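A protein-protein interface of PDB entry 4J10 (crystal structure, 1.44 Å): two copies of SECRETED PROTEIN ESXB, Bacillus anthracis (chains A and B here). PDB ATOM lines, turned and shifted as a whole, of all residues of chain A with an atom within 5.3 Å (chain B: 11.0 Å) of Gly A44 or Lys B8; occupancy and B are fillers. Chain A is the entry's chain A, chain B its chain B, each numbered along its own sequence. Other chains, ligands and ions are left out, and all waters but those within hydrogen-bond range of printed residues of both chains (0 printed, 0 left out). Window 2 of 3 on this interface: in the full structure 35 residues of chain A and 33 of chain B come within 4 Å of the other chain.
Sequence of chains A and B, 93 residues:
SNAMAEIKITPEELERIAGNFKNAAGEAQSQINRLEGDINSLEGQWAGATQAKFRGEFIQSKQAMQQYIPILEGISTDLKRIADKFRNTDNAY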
ATOM      1  N   LEU A  42      -7.566 -15.540 -17.763  1.00  0.00           N
ATOM      2  CA  LEU A  42      -6.497 -14.701 -17.220  1.00  0.00           C
ATOM      3  C   LEU A  42      -6.021 -13.626 -18.193  1.00  0.00           C
ATOM      4  O   LEU A  42      -5.321 -12.701 -17.800  1.00  0.00           O
ATOM      5  CB  LEU A  42      -5.308 -15.560 -16.798  1.00  0.00           C
ATOM      6  CG  LEU A  42      -5.595 -16.544 -15.662  1.00  0.00           C
ATOM      7  CD1 LEU A  42      -4.485 -17.570 -15.518  1.00  0.00           C
ATOM      8  CD2 LEU A  42      -5.795 -15.772 -14.365  1.00  0.00           C
ATOM      9  N   GLU A  43      -6.385 -13.760 -19.465  1.00  0.00           N
ATOM     10  CA  GLU A  43      -5.961 -12.797 -20.474  1.00  0.00           C
ATOM     11  C   GLU A  43      -6.424 -11.409 -20.079  1.00  0.00           C
ATOM     12  O   GLU A  43      -7.605 -11.196 -19.803  1.00  0.00           O
ATOM     13  CB  GLU A  43      -6.533 -13.165 -21.845  1.00  0.00           C
ATOM     14  CG  GLU A  43      -5.794 -12.529 -23.018  1.00  0.00           C
ATOM     15  CD  GLU A  43      -4.855 -13.501 -23.718  1.00  0.00           C
ATOM     16  OE1 GLU A  43      -4.067 -13.050 -24.575  1.00  0.00           O
ATOM     17  OE2 GLU A  43      -4.908 -14.715 -23.421  1.00  0.00           O
ATOM     18  N   GLY A  44      -5.479 -10.475 -20.021  1.00  0.00           N
ATOM     19  CA  GLY A  44      -5.789  -9.090 -19.715  1.00  0.00           C
ATOM     20  C   GLY A  44      -5.871  -8.764 -18.231  1.00  0.00           C
ATOM     21  O   GLY A  44      -5.999  -7.597 -17.858  1.00  0.00           O
ATOM     22  N   GLN A  45      -5.800  -9.794 -17.389  1.00  0.00           N
ATOM     23  CA  GLN A  45      -5.884  -9.629 -15.935  1.00  0.00           C
ATOM     24  C   GLN A  45      -4.510  -9.388 -15.298  1.00  0.00           C
ATOM     25  O   GLN A  45      -4.405  -9.160 -14.087  1.00  0.00           O
ATOM     26  CB  GLN A  45      -6.524 -10.871 -15.313  1.00  0.00           C
ATOM     27  CG  GLN A  45      -7.963 -11.112 -15.746  1.00  0.00           C
ATOM     28  CD  GLN A  45      -8.935 -10.203 -15.025  1.00  0.00           C
ATOM     29  OE1 GLN A  45      -9.219 -10.391 -13.839  1.00  0.00           O
ATOM     30  NE2 GLN A  45      -9.439  -9.200 -15.732  1.00  0.00           N
ATOM     31  N   TRP A  46      -3.469  -9.470 -16.123  1.00  0.00           N
ATOM     32  CA  TRP A  46      -2.086  -9.232 -15.710  1.00  0.00           C
ATOM     33  C   TRP A  46      -1.214  -9.005 -16.943  1.00  0.00           C
ATOM     34  O   TRP A  46      -1.721  -9.003 -18.061  1.00  0.00           O
ATOM     35  CB  TRP A  46      -1.533 -10.376 -14.841  1.00  0.00           C
ATOM     36  CG  TRP A  46      -1.633 -11.776 -15.419  1.00  0.00           C
ATOM     37  CD1 TRP A  46      -1.986 -12.129 -16.694  1.00  0.00           C
ATOM     38  CD2 TRP A  46      -1.384 -12.999 -14.721  1.00  0.00           C
ATOM     39  NE1 TRP A  46      -1.969 -13.495 -16.828  1.00  0.00           N
ATOM     40  CE2 TRP A  46      -1.599 -14.058 -15.630  1.00  0.00           C
ATOM     41  CE3 TRP A  46      -1.001 -13.318 -13.411  1.00  0.00           C
ATOM     42  CZ2 TRP A  46      -1.448 -15.397 -15.277  1.00  0.00           C
ATOM     43  CZ3 TRP A  46      -0.844 -14.643 -13.061  1.00  0.00           C
ATOM     44  CH2 TRP A  46      -1.067 -15.665 -13.988  1.00  0.00           C
ATOM     45  N   ILE B   7      -2.321  -5.040 -12.592  1.00  0.00           N
ATOM     46  CA  ILE B   7      -2.792  -6.353 -12.161  1.00  0.00           C
ATOM     47  C   ILE B   7      -4.234  -6.299 -11.675  1.00  0.00           C
ATOM     48  O   ILE B   7      -4.546  -5.580 -10.728  1.00  0.00           O
ATOM     49  CB  ILE B   7      -1.943  -6.915 -11.015  1.00  0.00           C
ATOM     50  CG1 ILE B   7      -0.449  -6.780 -11.322  1.00  0.00           C
ATOM     51  CG2 ILE B   7      -2.330  -8.357 -10.748  1.00  0.00           C
ATOM     52  CD1 ILE B   7       0.072  -7.776 -12.336  1.00  0.00           C
ATOM     53  N   LYS B   8      -5.104  -7.078 -12.308  1.00  0.00           N
ATOM     54  CA  LYS B   8      -6.520  -7.090 -11.958  1.00  0.00           C
ATOM     55  C   LYS B   8      -6.901  -8.335 -11.156  1.00  0.00           C
ATOM     56  O   LYS B   8      -7.861  -8.321 -10.381  1.00  0.00           O
ATOM     57  CB  LYS B   8      -7.372  -6.989 -13.225  1.00  0.00           C
ATOM     58  CG  LYS B   8      -7.178  -5.687 -13.985  1.00  0.00           C
ATOM     59  CD  LYS B   8      -7.971  -5.674 -15.279  1.00  0.00           C
ATOM     60  CE  LYS B   8      -7.844  -4.329 -15.975  1.00  0.00           C
ATOM     61  NZ  LYS B   8      -8.662  -4.264 -17.218  1.00  0.00           N
ATOM     62  N   ILE B   9      -6.140  -9.409 -11.342  1.00  0.00           N
ATOM     63  CA  ILE B   9      -6.430 -10.680 -10.692  1.00  0.00           C
ATOM     64  C   ILE B   9      -6.098 -10.686  -9.193  1.00  0.00           C
ATOM     65  O   ILE B   9      -5.109 -10.092  -8.770  1.00  0.00           O
ATOM     66  CB  ILE B   9      -5.690 -11.836 -11.412  1.00  0.00           C
ATOM     67  CG1 ILE B   9      -6.375 -13.164 -11.130  1.00  0.00           C
ATOM     68  CG2 ILE B   9      -4.202 -11.859 -11.079  1.00  0.00           C
ATOM     69  CD1 ILE B   9      -7.606 -13.344 -11.979  1.00  0.00           C
ATOM     70  N   THR B  10      -6.933 -11.349  -8.392  1.00  0.00           N
ATOM     71  CA  THR B  10      -6.661 -11.468  -6.959  1.00  0.00           C
ATOM     72  C   THR B  10      -5.875 -12.748  -6.660  1.00  0.00           C
ATOM     73  O   THR B  10      -5.930 -13.708  -7.428  1.00  0.00           O
ATOM     74  CB  THR B  10      -7.953 -11.491  -6.123  1.00  0.00           C
ATOM     75  OG1 THR B  10      -8.680 -12.692  -6.413  1.00  0.00           O
ATOM     76  CG2 THR B  10      -8.810 -10.242  -6.389  1.00  0.00           C
ATOM     77  N   PRO B  11      -5.134 -12.754  -5.532  1.00  0.00           N
ATOM     78  CA  PRO B  11      -4.420 -13.975  -5.149  1.00  0.00           C
ATOM     79  C   PRO B  11      -5.385 -15.138  -4.963  1.00  0.00           C
ATOM     80  O   PRO B  11      -5.068 -16.271  -5.330  1.00  0.00           O
ATOM     81  CB  PRO B  11      -3.767 -13.600  -3.818  1.00  0.00           C
ATOM     82  CG  PRO B  11      -3.661 -12.089  -3.844  1.00  0.00           C
ATOM     83  CD  PRO B  11      -4.838 -11.621  -4.635  1.00  0.00           C
ATOM     84  N   GLU B  12      -6.563 -14.859  -4.418  1.00  0.00           N
ATOM     85  CA  GLU B  12      -7.549 -15.908  -4.184  1.00  0.00           C
ATOM     86  C   GLU B  12      -7.992 -16.561  -5.497  1.00  0.00           C
ATOM     87  O   GLU B  12      -8.169 -17.786  -5.578  1.00  0.00           O
ATOM     88  CB  GLU B  12      -8.751 -15.338  -3.430  1.00  0.00           C
ATOM     89  CG  GLU B  12      -8.496 -15.034  -1.961  1.00  0.00           C
ATOM     90  CD  GLU B  12      -7.812 -13.700  -1.721  1.00  0.00           C
ATOM     91  OE1 GLU B  12      -7.592 -12.931  -2.685  1.00  0.00           O
ATOM     92  OE2 GLU B  12      -7.499 -13.408  -0.546  1.00  0.00           O
ATOM     93  N   GLU B  13      -8.152 -15.758  -6.542  1.00  0.00           N
ATOM     94  CA  GLU B  13      -8.565 -16.295  -7.833  1.00  0.00           C
ATOM     95  C   GLU B  13      -7.448 -17.111  -8.464  1.00  0.00           C
ATOM     96  O   GLU B  13      -7.701 -18.156  -9.081  1.00  0.00           O
ATOM     97  CB  GLU B  13      -9.031 -15.183  -8.781  1.00  0.00           C
ATOM     98  CG  GLU B  13      -9.317 -15.651 -10.211  1.00  0.00           C
ATOM     99  CD  GLU B  13     -10.598 -16.459 -10.366  1.00  0.00           C
ATOM    100  OE1 GLU B  13     -11.197 -16.871  -9.351  1.00  0.00           O
ATOM    101  OE2 GLU B  13     -11.009 -16.679 -11.527  1.00  0.00           O
ATOM    102  N   LEU B  14      -6.214 -16.642  -8.313  1.00  0.00           N
ATOM    103  CA  LEU B  14      -5.080 -17.412  -8.809  1.00  0.00           C
ATOM    104  C   LEU B  14      -5.032 -18.757  -8.090  1.00  0.00           C
ATOM    105  O   LEU B  14      -4.762 -19.784  -8.706  1.00  0.00           O
ATOM    106  CB  LEU B  14      -3.772 -16.645  -8.612  1.00  0.00           C
ATOM    107  CG  LEU B  14      -3.599 -15.416  -9.505  1.00  0.00           C
ATOM    108  CD1 LEU B  14      -2.351 -14.658  -9.130  1.00  0.00           C
ATOM    109  CD2 LEU B  14      -3.534 -15.866 -10.950  1.00  0.00           C
ATOM    110  N   ILE B  17      -7.791 -21.168  -9.509  1.00  0.00           N
ATOM    111  CA  ILE B  17      -7.367 -21.767 -10.764  1.00  0.00           C
ATOM    112  C   ILE B  17      -6.233 -22.765 -10.521  1.00  0.00           C
ATOM    113  O   ILE B  17      -6.208 -23.831 -11.135  1.00  0.00           O
ATOM    114  CB  ILE B  17      -6.988 -20.690 -11.803  1.00  0.00           C
ATOM    115  CG1 ILE B  17      -8.244 -19.914 -12.201  1.00  0.00           C
ATOM    116  CG2 ILE B  17      -6.341 -21.321 -13.031  1.00  0.00           C
ATOM    117  CD1 ILE B  17      -7.972 -18.624 -12.927  1.00  0.00           C
ATOM    118  N   ILE B  82       2.791 -17.040  -7.653  1.00  0.00           N
ATOM    119  CA  ILE B  82       2.421 -15.667  -7.981  1.00  0.00           C
ATOM    120  C   ILE B  82       1.388 -15.113  -7.006  1.00  0.00           C
ATOM    121  O   ILE B  82       1.508 -13.964  -6.571  1.00  0.00           O
ATOM    122  CB  ILE B  82       1.925 -15.537  -9.426  1.00  0.00           C
ATOM    123  CG1 ILE B  82       3.080 -15.811 -10.388  1.00  0.00           C
ATOM    124  CG2 ILE B  82       1.374 -14.145  -9.671  1.00  0.00           C
ATOM    125  CD1 ILE B  82       2.641 -16.039 -11.825  1.00  0.00           C
ATOM    126  N   PHE B  86       1.822 -11.745  -4.776  1.00  0.00           N
ATOM    127  CA  PHE B  86       0.842 -10.666  -4.857  1.00  0.00           C
ATOM    128  C   PHE B  86       0.286 -10.313  -3.484  1.00  0.00           C
ATOM    129  O   PHE B  86       0.156  -9.140  -3.140  1.00  0.00           O
ATOM    130  CB  PHE B  86      -0.325 -11.074  -5.762  1.00  0.00           C
ATOM    131  CG  PHE B  86      -0.033 -10.973  -7.234  1.00  0.00           C
ATOM    132  CD1 PHE B  86       1.220 -10.595  -7.695  1.00  0.00           C
ATOM    133  CD2 PHE B  86      -1.029 -11.250  -8.161  1.00  0.00           C
ATOM    134  CE1 PHE B  86       1.474 -10.503  -9.057  1.00  0.00           C
ATOM    135  CE2 PHE B  86      -0.782 -11.157  -9.519  1.00  0.00           C
ATOM    136  CZ  PHE B  86       0.468 -10.783  -9.968  1.00  0.00           C
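No residue of chain B comes within 4 Å of Glu A43.
Gly A44 touches just one residue of chain B: Lys B8.
Gln A45 touches just these residues of chain B: Ile B7 (3.7 Å), Lys B8 (2.8 Å) and Ile B9 (3.3 Å).
Printed residues of chain B within 4 Å of Trp A46: Ile B7, Leu B14 and Ile B82.
Printed residues of chain A within 4 Å of Ile B7: Gln A45 (3.7 Å) and Trp A46 (3.95 Å).
Of chain A, only Gly A44 and Gln A45 come within 4 Å of Lys B8.
Of the printed residues of chain A, Ile B9 touches Leu A42 and Gln A45.
Of the printed residues of chain A, Leu B14 touches Trp A46.
Of the printed residues of chain A, Ile B82 touches Trp A46 (3.95 Å).
The nearest residue of chain B that does not touch Gly A44 is Ile B7 (6.6 Å).
The nearest residue of chain A that does not touch Lys B8 is Trp A46 (4.8 Å).
No position is printed for both chains.
O of Gln A45 lies within hydrogen-bond range of N of Lys B8, at 2.8 Å.
The backbone NH of Ile B9 sits at hydrogen-bond distance from the backbone carbonyl oxygen of Gln A45 (3.3 Å).
Of the 11 printed residues of chain B, 6 touch a printed residue of chain A.
Hydrophobic or aromatic side chains of chain B that line the printed part of chain A: Ile B7, Ile B9, Leu B14, Ile B17 and Ile B82.
Of the 5 printed residues of chain A, 4 touch a printed residue of chain B.
Hydrophobic or aromatic side chains of chain A within 4 Å of the printed part of chain B: Leu A42 and Trp A46.
Among the printed residues, no Asp or Glu carboxylate lies within 4 Å of a Lys or Arg side-chain nitrogen of the other chain.
Leu A42 touches Ile B9 (CD2 to CD1, 3.9 Å).
Leu A42 touches Ile B17.
Gly A44 touches Lys B8.
Ile B7 touches Gln A45 (C to O, 3.7 Å).
CD1 of Ile B7 touches CB of Trp A46 (3.95 Å).
Trp A46 touches Leu B14 (CZ3 to CD2, 3.6 Å).
Trp A46 touches Ile B82 (CZ3 to CD1, 3.95 Å).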
